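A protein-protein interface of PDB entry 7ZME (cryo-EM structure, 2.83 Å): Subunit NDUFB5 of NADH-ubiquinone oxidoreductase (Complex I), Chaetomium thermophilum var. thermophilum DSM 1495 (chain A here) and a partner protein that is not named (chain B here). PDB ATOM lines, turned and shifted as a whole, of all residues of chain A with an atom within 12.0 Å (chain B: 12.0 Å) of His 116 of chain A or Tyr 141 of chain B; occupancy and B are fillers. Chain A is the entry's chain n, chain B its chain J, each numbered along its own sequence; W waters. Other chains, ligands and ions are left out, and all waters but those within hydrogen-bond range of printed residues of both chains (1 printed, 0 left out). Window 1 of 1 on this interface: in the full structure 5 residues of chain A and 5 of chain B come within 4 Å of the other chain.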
ATOM      1  N   ALA A 107     -25.529 -41.491 -16.675  1.00  0.00           N
ATOM      2  CA  ALA A 107     -24.680 -40.562 -17.411  1.00  0.00           C
ATOM      3  C   ALA A 107     -25.292 -39.171 -17.454  1.00  0.00           C
ATOM      4  O   ALA A 107     -24.574 -38.167 -17.422  1.00  0.00           O
ATOM      5  CB  ALA A 107     -24.432 -41.089 -18.824  1.00  0.00           C
ATOM      6  N   LEU A 108     -26.618 -39.092 -17.518  1.00  0.00           N
ATOM      7  CA  LEU A 108     -27.311 -37.812 -17.534  1.00  0.00           C
ATOM      8  C   LEU A 108     -27.659 -37.298 -16.144  1.00  0.00           C
ATOM      9  O   LEU A 108     -27.874 -36.093 -15.988  1.00  0.00           O
ATOM     10  CB  LEU A 108     -28.571 -37.922 -18.396  1.00  0.00           C
ATOM     11  CG  LEU A 108     -28.201 -38.240 -19.846  1.00  0.00           C
ATOM     12  CD1 LEU A 108     -29.383 -38.730 -20.632  1.00  0.00           C
ATOM     13  CD2 LEU A 108     -27.609 -37.009 -20.499  1.00  0.00           C
ATOM     14  N   GLU A 109     -27.732 -38.173 -15.136  1.00  0.00           N
ATOM     15  CA  GLU A 109     -27.690 -37.707 -13.753  1.00  0.00           C
ATOM     16  C   GLU A 109     -26.408 -36.935 -13.481  1.00  0.00           C
ATOM     17  O   GLU A 109     -26.435 -35.830 -12.930  1.00  0.00           O
ATOM     18  CB  GLU A 109     -27.794 -38.883 -12.779  1.00  0.00           C
ATOM     19  CG  GLU A 109     -29.098 -39.656 -12.740  1.00  0.00           C
ATOM     20  CD  GLU A 109     -30.252 -38.837 -12.205  1.00  0.00           C
ATOM     21  OE1 GLU A 109     -30.016 -37.959 -11.349  1.00  0.00           O
ATOM     22  OE2 GLU A 109     -31.402 -39.112 -12.595  1.00  0.00           O
ATOM     23  N   GLN A 110     -25.266 -37.517 -13.853  1.00  0.00           N
ATOM     24  CA  GLN A 110     -23.982 -36.896 -13.554  1.00  0.00           C
ATOM     25  C   GLN A 110     -23.807 -35.592 -14.319  1.00  0.00           C
ATOM     26  O   GLN A 110     -23.267 -34.619 -13.781  1.00  0.00           O
ATOM     27  CB  GLN A 110     -22.844 -37.865 -13.870  1.00  0.00           C
ATOM     28  CG  GLN A 110     -22.859 -39.118 -13.017  1.00  0.00           C
ATOM     29  CD  GLN A 110     -22.594 -38.828 -11.553  1.00  0.00           C
ATOM     30  OE1 GLN A 110     -21.767 -37.981 -11.215  1.00  0.00           O
ATOM     31  NE2 GLN A 110     -23.299 -39.530 -10.674  1.00  0.00           N
ATOM     32  N   ALA A 111     -24.292 -35.577 -15.561  1.00  0.00           N
ATOM     33  CA  ALA A 111     -24.308 -34.343 -16.374  1.00  0.00           C
ATOM     34  C   ALA A 111     -25.016 -33.253 -15.577  1.00  0.00           C
ATOM     35  O   ALA A 111     -24.460 -32.153 -15.456  1.00  0.00           O
ATOM     36  CB  ALA A 111     -25.006 -34.605 -17.677  1.00  0.00           C
ATOM     37  N   ALA A 112     -26.216 -33.555 -15.076  1.00  0.00           N
ATOM     38  CA  ALA A 112     -27.043 -32.551 -14.369  1.00  0.00           C
ATOM     39  C   ALA A 112     -26.340 -32.038 -13.111  1.00  0.00           C
ATOM     40  O   ALA A 112     -26.428 -30.832 -12.849  1.00  0.00           O
ATOM     41  CB  ALA A 112     -28.391 -33.139 -14.046  1.00  0.00           C
ATOM     42  N   HIS A 113     -25.675 -32.921 -12.370  1.00  0.00           N
ATOM     43  CA  HIS A 113     -24.947 -32.497 -11.154  1.00  0.00           C
ATOM     44  C   HIS A 113     -23.854 -31.510 -11.555  1.00  0.00           C
ATOM     45  O   HIS A 113     -23.719 -30.481 -10.882  1.00  0.00           O
ATOM     46  CB  HIS A 113     -24.368 -33.729 -10.448  1.00  0.00           C
ATOM     47  CG  HIS A 113     -23.505 -33.405  -9.275  1.00  0.00           C
ATOM     48  ND1 HIS A 113     -23.979 -33.442  -7.980  1.00  0.00           N
ATOM     49  CD2 HIS A 113     -22.208 -33.037  -9.193  1.00  0.00           C
ATOM     50  CE1 HIS A 113     -23.012 -33.110  -7.152  1.00  0.00           C
ATOM     51  NE2 HIS A 113     -21.916 -32.854  -7.871  1.00  0.00           N
ATOM     52  N   ASP A 114     -23.129 -31.811 -12.629  1.00  0.00           N
ATOM     53  CA  ASP A 114     -22.029 -30.932 -13.100  1.00  0.00           C
ATOM     54  C   ASP A 114     -22.603 -29.588 -13.529  1.00  0.00           C
ATOM     55  O   ASP A 114     -22.034 -28.555 -13.148  1.00  0.00           O
ATOM     56  CB  ASP A 114     -21.301 -31.574 -14.278  1.00  0.00           C
ATOM     57  CG  ASP A 114     -20.645 -32.898 -13.929  1.00  0.00           C
ATOM     58  OD1 ASP A 114     -20.525 -33.194 -12.723  1.00  0.00           O
ATOM     59  OD2 ASP A 114     -20.265 -33.628 -14.866  1.00  0.00           O
ATOM     60  N   LYS A 115     -23.710 -29.618 -14.266  1.00  0.00           N
ATOM     61  CA  LYS A 115     -24.312 -28.370 -14.783  1.00  0.00           C
ATOM     62  C   LYS A 115     -24.750 -27.545 -13.588  1.00  0.00           C
ATOM     63  O   LYS A 115     -24.510 -26.332 -13.588  1.00  0.00           O
ATOM     64  CB  LYS A 115     -25.514 -28.719 -15.665  1.00  0.00           C
ATOM     65  CG  LYS A 115     -26.181 -27.547 -16.372  1.00  0.00           C
ATOM     66  CD  LYS A 115     -27.393 -27.960 -17.181  1.00  0.00           C
ATOM     67  CE  LYS A 115     -27.968 -26.830 -18.006  1.00  0.00           C
ATOM     68  NZ  LYS A 115     -28.378 -25.685 -17.160  1.00  0.00           N
ATOM     69  N   HIS A 116     -25.342 -28.205 -12.597  1.00  0.00           N
ATOM     70  CA  HIS A 116     -25.843 -27.493 -11.396  1.00  0.00           C
ATOM     71  C   HIS A 116     -24.663 -26.855 -10.666  1.00  0.00           C
ATOM     72  O   HIS A 116     -24.725 -25.659 -10.424  1.00  0.00           O
ATOM     73  CB  HIS A 116     -26.677 -28.481 -10.586  1.00  0.00           C
ATOM     74  CG  HIS A 116     -26.953 -28.097  -9.178  1.00  0.00           C
ATOM     75  ND1 HIS A 116     -27.267 -29.034  -8.220  1.00  0.00           N
ATOM     76  CD2 HIS A 116     -26.980 -26.901  -8.563  1.00  0.00           C
ATOM     77  CE1 HIS A 116     -27.454 -28.434  -7.071  1.00  0.00           C
ATOM     78  NE2 HIS A 116     -27.286 -27.128  -7.259  1.00  0.00           N
ATOM     79  N   LEU A 117     -23.575 -27.592 -10.489  1.00  0.00           N
ATOM     80  CA  LEU A 117     -22.387 -27.080  -9.773  1.00  0.00           C
ATOM     81  C   LEU A 117     -21.802 -25.872 -10.519  1.00  0.00           C
ATOM     82  O   LEU A 117     -21.353 -24.934  -9.844  1.00  0.00           O
ATOM     83  CB  LEU A 117     -21.390 -28.237  -9.673  1.00  0.00           C
ATOM     84  CG  LEU A 117     -20.124 -27.963  -8.871  1.00  0.00           C
ATOM     85  CD1 LEU A 117     -20.419 -28.004  -7.382  1.00  0.00           C
ATOM     86  CD2 LEU A 117     -19.046 -28.970  -9.227  1.00  0.00           C
ATOM     87  N   LEU A 118     -21.799 -25.901 -11.855  1.00  0.00           N
ATOM     88  CA  LEU A 118     -21.230 -24.800 -12.672  1.00  0.00           C
ATOM     89  C   LEU A 118     -22.139 -23.556 -12.682  1.00  0.00           C
ATOM     90  O   LEU A 118     -21.589 -22.464 -12.487  1.00  0.00           O
ATOM     91  CB  LEU A 118     -20.939 -25.314 -14.086  1.00  0.00           C
ATOM     92  CG  LEU A 118     -19.794 -26.316 -14.221  1.00  0.00           C
ATOM     93  CD1 LEU A 118     -19.920 -27.106 -15.512  1.00  0.00           C
ATOM     94  CD2 LEU A 118     -18.446 -25.621 -14.155  1.00  0.00           C
ATOM     95  N   LEU A 119     -23.452 -23.682 -12.916  1.00  0.00           N
ATOM     96  CA  LEU A 119     -24.280 -22.483 -12.977  1.00  0.00           C
ATOM     97  C   LEU A 119     -24.580 -21.900 -11.604  1.00  0.00           C
ATOM     98  O   LEU A 119     -24.900 -20.712 -11.511  1.00  0.00           O
ATOM     99  CB  LEU A 119     -25.586 -22.758 -13.724  1.00  0.00           C
ATOM    100  CG  LEU A 119     -25.540 -22.810 -15.255  1.00  0.00           C
ATOM    101  CD1 LEU A 119     -24.843 -24.044 -15.798  1.00  0.00           C
ATOM    102  CD2 LEU A 119     -26.953 -22.718 -15.801  1.00  0.00           C
ATOM    103  N   THR A 120     -24.485 -22.694 -10.544  1.00  0.00           N
ATOM    104  CA  THR A 120     -24.694 -22.202  -9.193  1.00  0.00           C
ATOM    105  C   THR A 120     -23.395 -21.800  -8.516  1.00  0.00           C
ATOM    106  O   THR A 120     -23.399 -21.516  -7.315  1.00  0.00           O
ATOM    107  CB  THR A 120     -25.414 -23.249  -8.346  1.00  0.00           C
ATOM    108  OG1 THR A 120     -24.626 -24.444  -8.296  1.00  0.00           O
ATOM    109  CG2 THR A 120     -26.777 -23.568  -8.932  1.00  0.00           C
ATOM    110  N   ALA A 121     -22.288 -21.780  -9.255  1.00  0.00           N
ATOM    111  CA  ALA A 121     -21.007 -21.398  -8.678  1.00  0.00           C
ATOM    112  C   ALA A 121     -21.069 -19.977  -8.144  1.00  0.00           C
ATOM    113  O   ALA A 121     -21.644 -19.084  -8.769  1.00  0.00           O
ATOM    114  CB  ALA A 121     -19.895 -21.526  -9.717  1.00  0.00           C
ATOM    115  N   GLU A 122     -20.482 -19.777  -6.969  1.00  0.00           N
ATOM    116  CA  GLU A 122     -20.549 -18.483  -6.304  1.00  0.00           C
ATOM    117  C   GLU A 122     -19.813 -17.426  -7.114  1.00  0.00           C
ATOM    118  O   GLU A 122     -18.716 -17.667  -7.624  1.00  0.00           O
ATOM    119  CB  GLU A 122     -19.958 -18.586  -4.901  1.00  0.00           C
ATOM    120  CG  GLU A 122     -20.250 -19.908  -4.210  1.00  0.00           C
ATOM    121  CD  GLU A 122     -19.835 -19.912  -2.753  1.00  0.00           C
ATOM    122  OE1 GLU A 122     -18.923 -19.140  -2.392  1.00  0.00           O
ATOM    123  OE2 GLU A 122     -20.420 -20.689  -1.971  1.00  0.00           O
ATOM    124  N   ARG A 123     -20.427 -16.256  -7.239  1.00  0.00           N
ATOM    125  CA  ARG A 123     -19.798 -15.138  -7.924  1.00  0.00           C
ATOM    126  C   ARG A 123     -18.830 -14.433  -6.987  1.00  0.00           C
ATOM    127  O   ARG A 123     -19.172 -14.109  -5.846  1.00  0.00           O
ATOM    128  CB  ARG A 123     -20.857 -14.157  -8.422  1.00  0.00           C
ATOM    129  CG  ARG A 123     -20.305 -12.838  -8.907  1.00  0.00           C
ATOM    130  CD  ARG A 123     -21.377 -11.779  -8.895  1.00  0.00           C
ATOM    131  NE  ARG A 123     -21.025 -10.630  -9.720  1.00  0.00           N
ATOM    132  CZ  ARG A 123     -21.688 -10.263 -10.809  1.00  0.00           C
ATOM    133  NH1 ARG A 123     -22.738 -10.959 -11.210  1.00  0.00           N
ATOM    134  NH2 ARG A 123     -21.298  -9.204 -11.497  1.00  0.00           N
ATOM    135  N   ARG A 125     -16.707 -11.574  -5.274  1.00  0.00           N
ATOM    136  CA  ARG A 125     -16.925 -10.136  -4.996  1.00  0.00           C
ATOM    137  C   ARG A 125     -15.580  -9.469  -4.690  1.00  0.00           C
ATOM    138  O   ARG A 125     -15.590  -8.312  -4.251  1.00  0.00           O
ATOM    139  CB  ARG A 125     -17.935  -9.986  -3.855  1.00  0.00           C
ATOM    140  CG  ARG A 125     -17.665 -10.892  -2.663  1.00  0.00           C
ATOM    141  CD  ARG A 125     -18.896 -11.014  -1.787  1.00  0.00           C
ATOM    142  NE  ARG A 125     -19.983 -11.706  -2.462  1.00  0.00           N
ATOM    143  CZ  ARG A 125     -21.167 -11.957  -1.916  1.00  0.00           C
ATOM    144  NH1 ARG A 125     -21.418 -11.569  -0.677  1.00  0.00           N
ATOM    145  NH2 ARG A 125     -22.093 -12.593  -2.609  1.00  0.00           N
ATOM    146  N   ARG B 136     -31.564 -13.698  -3.127  1.00  0.00           N
ATOM    147  CA  ARG B 136     -31.781 -14.936  -2.385  1.00  0.00           C
ATOM    148  C   ARG B 136     -31.071 -14.908  -1.037  1.00  0.00           C
ATOM    149  O   ARG B 136     -31.632 -15.344  -0.024  1.00  0.00           O
ATOM    150  CB  ARG B 136     -31.316 -16.131  -3.214  1.00  0.00           C
ATOM    151  N   ASP B 137     -29.833 -14.411  -1.009  1.00  0.00           N
ATOM    152  CA  ASP B 137     -29.005 -14.350   0.196  1.00  0.00           C
ATOM    153  C   ASP B 137     -28.740 -15.731   0.789  1.00  0.00           C
ATOM    154  O   ASP B 137     -28.346 -15.846   1.954  1.00  0.00           O
ATOM    155  CB  ASP B 137     -29.624 -13.432   1.256  1.00  0.00           C
ATOM    156  CG  ASP B 137     -29.999 -12.074   0.702  1.00  0.00           C
ATOM    157  OD1 ASP B 137     -29.314 -11.599  -0.228  1.00  0.00           O
ATOM    158  OD2 ASP B 137     -30.982 -11.479   1.193  1.00  0.00           O
ATOM    159  N   VAL B 138     -28.951 -16.788   0.002  1.00  0.00           N
ATOM    160  CA  VAL B 138     -28.738 -18.159   0.439  1.00  0.00           C
ATOM    161  C   VAL B 138     -27.992 -18.907  -0.656  1.00  0.00           C
ATOM    162  O   VAL B 138     -27.889 -18.449  -1.796  1.00  0.00           O
ATOM    163  CB  VAL B 138     -30.059 -18.882   0.780  1.00  0.00           C
ATOM    164  CG1 VAL B 138     -30.627 -18.363   2.092  1.00  0.00           C
ATOM    165  CG2 VAL B 138     -31.062 -18.709  -0.349  1.00  0.00           C
ATOM    166  N   ASP B 139     -27.464 -20.075  -0.290  1.00  0.00           N
ATOM    167  CA  ASP B 139     -26.743 -20.913  -1.237  1.00  0.00           C
ATOM    168  C   ASP B 139     -27.658 -21.368  -2.364  1.00  0.00           C
ATOM    169  O   ASP B 139     -28.579 -22.160  -2.145  1.00  0.00           O
ATOM    170  CB  ASP B 139     -26.138 -22.127  -0.530  1.00  0.00           C
ATOM    171  CG  ASP B 139     -25.173 -22.894  -1.410  1.00  0.00           C
ATOM    172  OD1 ASP B 139     -24.582 -22.279  -2.324  1.00  0.00           O
ATOM    173  OD2 ASP B 139     -25.006 -24.112  -1.191  1.00  0.00           O
ATOM    174  N   GLU B 140     -27.387 -20.889  -3.580  1.00  0.00           N
ATOM    175  CA  GLU B 140     -28.209 -21.277  -4.756  1.00  0.00           C
ATOM    176  C   GLU B 140     -27.970 -22.756  -5.052  1.00  0.00           C
ATOM    177  O   GLU B 140     -28.891 -23.416  -5.557  1.00  0.00           O
ATOM    178  CB  GLU B 140     -27.839 -20.424  -5.971  1.00  0.00           C
ATOM    179  N   TYR B 141     -26.771 -23.245  -4.740  1.00  0.00           N
ATOM    180  CA  TYR B 141     -26.442 -24.663  -5.018  1.00  0.00           C
ATOM    181  C   TYR B 141     -27.369 -25.563  -4.207  1.00  0.00           C
ATOM    182  O   TYR B 141     -27.892 -26.543  -4.733  1.00  0.00           O
ATOM    183  CB  TYR B 141     -24.977 -24.960  -4.700  1.00  0.00           C
ATOM    184  CG  TYR B 141     -24.571 -26.393  -4.924  1.00  0.00           C
ATOM    185  CD1 TYR B 141     -24.163 -26.832  -6.171  1.00  0.00           C
ATOM    186  CD2 TYR B 141     -24.600 -27.316  -3.892  1.00  0.00           C
ATOM    187  CE1 TYR B 141     -23.800 -28.148  -6.390  1.00  0.00           C
ATOM    188  CE2 TYR B 141     -24.238 -28.637  -4.092  1.00  0.00           C
ATOM    189  CZ  TYR B 141     -23.834 -29.054  -5.346  1.00  0.00           C
ATOM    190  OH  TYR B 141     -23.472 -30.352  -5.554  1.00  0.00           O
ATOM    191  N   GLU B 142     -27.616 -25.214  -2.951  1.00  0.00           N
ATOM    192  CA  GLU B 142     -28.423 -26.155  -2.144  1.00  0.00           C
ATOM    193  C   GLU B 142     -29.902 -25.922  -2.451  1.00  0.00           C
ATOM    194  O   GLU B 142     -30.669 -26.880  -2.293  1.00  0.00           O
ATOM    195  CB  GLU B 142     -28.094 -25.987  -0.660  1.00  0.00           C
ATOM    196  CG  GLU B 142     -28.658 -27.094   0.212  1.00  0.00           C
ATOM    197  CD  GLU B 142     -28.337 -28.500  -0.267  1.00  0.00           C
ATOM    198  OE1 GLU B 142     -27.153 -28.772  -0.551  1.00  0.00           O
ATOM    199  OE2 GLU B 142     -29.275 -29.317  -0.366  1.00  0.00           O
ATOM    200  N   ARG B 143     -30.290 -24.741  -2.933  1.00  0.00           N
ATOM    201  CA  ARG B 143     -31.728 -24.608  -3.269  1.00  0.00           C
ATOM    202  C   ARG B 143     -32.063 -25.523  -4.449  1.00  0.00           C
ATOM    203  O   ARG B 143     -33.086 -26.214  -4.386  1.00  0.00           O
ATOM    204  CB  ARG B 143     -32.044 -23.156  -3.632  1.00  0.00           C
ATOM    205  CG  ARG B 143     -33.492 -22.913  -4.034  1.00  0.00           C
ATOM    206  CD  ARG B 143     -33.728 -21.478  -4.463  1.00  0.00           C
ATOM    207  NE  ARG B 143     -32.840 -21.065  -5.540  1.00  0.00           N
ATOM    208  CZ  ARG B 143     -33.133 -21.136  -6.834  1.00  0.00           C
ATOM    209  NH1 ARG B 143     -34.306 -21.604  -7.225  1.00  0.00           N
ATOM    210  NH2 ARG B 143     -32.252 -20.733  -7.732  1.00  0.00           N
ATOM    211  N   LYS B 144     -31.207 -25.563  -5.466  1.00  0.00           N
ATOM    212  CA  LYS B 144     -31.411 -26.439  -6.648  1.00  0.00           C
ATOM    213  C   LYS B 144     -31.379 -27.900  -6.211  1.00  0.00           C
ATOM    214  O   LYS B 144     -32.290 -28.646  -6.602  1.00  0.00           O
ATOM    215  CB  LYS B 144     -30.382 -26.131  -7.735  1.00  0.00           C
ATOM    216  CG  LYS B 144     -30.546 -24.787  -8.428  1.00  0.00           C
ATOM    217  CD  LYS B 144     -31.881 -24.635  -9.115  1.00  0.00           C
ATOM    218  CE  LYS B 144     -31.908 -23.475 -10.089  1.00  0.00           C
ATOM    219  NZ  LYS B 144     -30.977 -23.692 -11.221  1.00  0.00           N
ATOM    220  N   GLU B 145     -30.361 -28.293  -5.442  1.00  0.00           N
ATOM    221  CA  GLU B 145     -30.207 -29.709  -5.015  1.00  0.00           C
ATOM    222  C   GLU B 145     -31.421 -30.153  -4.195  1.00  0.00           C
ATOM    223  O   GLU B 145     -31.916 -31.267  -4.441  1.00  0.00           O
ATOM    224  CB  GLU B 145     -28.960 -29.842  -4.143  1.00  0.00           C
ATOM    225  CG  GLU B 145     -28.414 -31.257  -4.065  1.00  0.00           C
ATOM    226  CD  GLU B 145     -27.651 -31.723  -5.294  1.00  0.00           C
ATOM    227  OE1 GLU B 145     -28.299 -32.047  -6.309  1.00  0.00           O
ATOM    228  OE2 GLU B 145     -26.407 -31.763  -5.231  1.00  0.00           O
ATOM    229  N   PHE B 146     -31.894 -29.305  -3.281  1.00  0.00           N
ATOM    230  CA  PHE B 146     -33.015 -29.708  -2.398  1.00  0.00           C
ATOM    231  C   PHE B 146     -34.266 -29.976  -3.234  1.00  0.00           C
ATOM    232  O   PHE B 146     -34.908 -31.006  -3.006  1.00  0.00           O
ATOM    233  CB  PHE B 146     -33.278 -28.623  -1.352  1.00  0.00           C
ATOM    234  CG  PHE B 146     -34.586 -28.765  -0.615  1.00  0.00           C
ATOM    235  CD1 PHE B 146     -34.783 -29.801   0.285  1.00  0.00           C
ATOM    236  CD2 PHE B 146     -35.618 -27.865  -0.820  1.00  0.00           C
ATOM    237  CE1 PHE B 146     -35.987 -29.934   0.959  1.00  0.00           C
ATOM    238  CE2 PHE B 146     -36.821 -27.999  -0.144  1.00  0.00           C
ATOM    239  CZ  PHE B 146     -37.002 -29.031   0.745  1.00  0.00           C
ATOM    240  N   LEU B 147     -34.576 -29.092  -4.182  1.00  0.00           N
ATOM    241  CA  LEU B 147     -35.795 -29.248  -5.020  1.00  0.00           C
ATOM    242  C   LEU B 147     -35.673 -30.494  -5.897  1.00  0.00           C
ATOM    243  O   LEU B 147     -36.663 -31.234  -5.999  1.00  0.00           O
ATOM    244  CB  LEU B 147     -35.951 -27.991  -5.879  1.00  0.00           C
ATOM    245  CG  LEU B 147     -36.329 -26.715  -5.133  1.00  0.00           C
ATOM    246  CD1 LEU B 147     -36.337 -25.525  -6.078  1.00  0.00           C
ATOM    247  CD2 LEU B 147     -37.681 -26.866  -4.456  1.00  0.00           C
ATOM    248  N   ARG B 148     -34.503 -30.715  -6.492  1.00  0.00           N
ATOM    249  CA  ARG B 148     -34.280 -31.846  -7.425  1.00  0.00           C
ATOM    250  C   ARG B 148     -34.328 -33.214  -6.739  1.00  0.00           C
ATOM    251  O   ARG B 148     -34.896 -34.144  -7.343  1.00  0.00           O
ATOM    252  CB  ARG B 148     -32.925 -31.612  -8.098  1.00  0.00           C
ATOM    253  CG  ARG B 148     -32.405 -32.750  -8.959  1.00  0.00           C
ATOM    254  CD  ARG B 148     -31.056 -32.283  -9.463  1.00  0.00           C
ATOM    255  NE  ARG B 148     -31.076 -30.831  -9.578  1.00  0.00           N
ATOM    256  CZ  ARG B 148     -30.172 -30.113 -10.228  1.00  0.00           C
ATOM    257  NH1 ARG B 148     -30.282 -28.796 -10.277  1.00  0.00           N
ATOM    258  NH2 ARG B 148     -29.171 -30.716 -10.842  1.00  0.00           N
ATOM    259  N   LYS B 149     -33.704 -33.327  -5.562  1.00  0.00           N
ATOM    260  CA  LYS B 149     -33.573 -34.646  -4.892  1.00  0.00           C
ATOM    261  C   LYS B 149     -34.725 -34.882  -3.920  1.00  0.00           C
ATOM    262  O   LYS B 149     -34.810 -36.005  -3.388  1.00  0.00           O
ATOM    263  CB  LYS B 149     -32.198 -34.762  -4.229  1.00  0.00           C
ATOM    264  CG  LYS B 149     -31.019 -34.729  -5.192  1.00  0.00           C
ATOM    265  CD  LYS B 149     -29.693 -35.000  -4.517  1.00  0.00           C
ATOM    266  CE  LYS B 149     -29.653 -36.342  -3.818  1.00  0.00           C
ATOM    267  NZ  LYS B 149     -28.340 -36.586  -3.176  1.00  0.00           N
ATOM    268  N   ASN B 150     -35.586 -33.885  -3.705  1.00  0.00           N
ATOM    269  CA  ASN B 150     -36.777 -34.184  -2.871  1.00  0.00           C
ATOM    270  C   ASN B 150     -37.700 -34.959  -3.808  1.00  0.00           C
ATOM    271  O   ASN B 150     -38.248 -34.338  -4.739  1.00  0.00           O
ATOM    272  CB  ASN B 150     -37.452 -32.917  -2.347  1.00  0.00           C
ATOM    273  CG  ASN B 150     -38.697 -33.196  -1.533  1.00  0.00           C
ATOM    274  OD1 ASN B 150     -38.843 -34.270  -0.953  1.00  0.00           O
ATOM    275  ND2 ASN B 150     -39.599 -32.229  -1.476  1.00  0.00           N
ATOM    276  N   ARG B 151     -37.867 -36.259  -3.569  1.00  0.00           N
ATOM    277  CA  ARG B 151     -38.645 -37.088  -4.525  1.00  0.00           C
ATOM    278  C   ARG B 151     -39.851 -37.695  -3.811  1.00  0.00           C
ATOM    279  O   ARG B 151     -40.836 -38.008  -4.500  1.00  0.00           O
ATOM    280  CB  ARG B 151     -37.733 -38.140  -5.164  1.00  0.00           C
ATOM    281  CG  ARG B 151     -36.688 -37.556  -6.102  1.00  0.00           C
ATOM    282  CD  ARG B 151     -35.887 -38.617  -6.832  1.00  0.00           C
ATOM    283  NE  ARG B 151     -34.918 -38.058  -7.758  1.00  0.00           N
ATOM    284  CZ  ARG B 151     -33.664 -37.760  -7.439  1.00  0.00           C
ATOM    285  NH1 ARG B 151     -32.850 -37.253  -8.348  1.00  0.00           N
ATOM    286  NH2 ARG B 151     -33.230 -37.965  -6.209  1.00  0.00           N
HETATM  287  O   HOH W   1     -25.331 -30.457  -8.280  1.00  0.00           O
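OD1 of Asp 139 of chain B sits close to N of Tyr 141 of chain B (3.4 Å). The side-chain carboxylate (OE2) of Glu 145 of chain B lies within hydrogen-bond range of the side-chain hydroxyl (OH) of Tyr 141 of chain B (3.3 Å). O of His 116 of chain A is in hydrogen-bond range of OG1 of Thr 120 of chain A (2.5 Å).
Among the printed residues, merely in contact across the chains: His 113 of chain A with Tyr 141 of chain B (3.2 Å), His 116 of chain A with Lys 144 of chain B (3.3 Å), His 116 of chain A with Glu 145 of chain B (3.3 Å), His 116 of chain A with Arg 148 of chain B (3.4 Å), Leu 117 of chain A with Tyr 141 of chain B (3.5 Å), Thr 120 of chain A with Glu 140 of chain B (3.99 Å), Thr 120 of chain A with Tyr 141 of chain B (3.2 Å) and Thr 120 of chain A with Lys 144 of chain B (3.99 Å).
Hydrophobic or aromatic side chains of chain A that line the printed part of chain B: His 113, His 116 and Leu 117. Of the 16 printed residues of chain B, 5 touch a printed residue of chain A.
The backbone carbonyl oxygen of Tyr 141 of chain B lies within hydrogen-bond range of a ring nitrogen (NE2) of His 116 of chain A, 2.7 Å away. NH2 of Arg 148 of chain B sits at hydrogen-bond distance from O of Ala 112 of chain A (3.4 Å).
Water W1 lies within hydrogen-bond range of ND1 of His 116 of chain A, O of His 113 of chain A, OH of Tyr 141 of chain B and OE2 of Glu 145 of chain B.
Of chain B, only Arg 148 (3.4 Å) comes within 4 Å of Ala 112 of chain A. His 113 of chain A touches one residue of chain B. No residue of chain B comes within 4 Å of Asp 114 of chain A. His 116 of chain A touches just these residues of chain B: Tyr 141, Lys 144, Glu 145 and Arg 148. Of the printed residues of chain B, Leu 117 of chain A touches Tyr 141 (3.5 Å). Leu 118 of chain A touches none of the printed residues of chain B. Printed residues of chain B within 4 Å of Thr 120 of chain A: Glu 140 (3.99 Å), Tyr 141 (3.2 Å) and Lys 144 (3.99 Å). No residue of chain B comes within 4 Å of Ala 121 of chain A. No residue of chain A comes within 4 Å of Asp 139 of chain B. Of the printed residues of chain A, Glu 140 of chain B touches Thr 120. Tyr 141 of chain B touches just these residues of chain A: His 113 (3.2 Å), His 116 (2.7 Å), Leu 117 (3.5 Å) and Thr 120 (3.2 Å). Glu 142 of chain B touches none of the printed residues of chain A. Of the printed residues of chain A, Lys 144 of chain B touches His 116 (3.3 Å) and Thr 120 (3.99 Å). Printed residues of chain A within 4 Å of Arg 148 of chain B: Ala 112 and His 116. The nearest residue of chain B that does not touch His 116 of chain A is Glu 140 of chain B (4.4 Å). The nearest residue of chain A that does not touch Tyr 141 of chain B is Ala 121 of chain A (6.2 Å).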
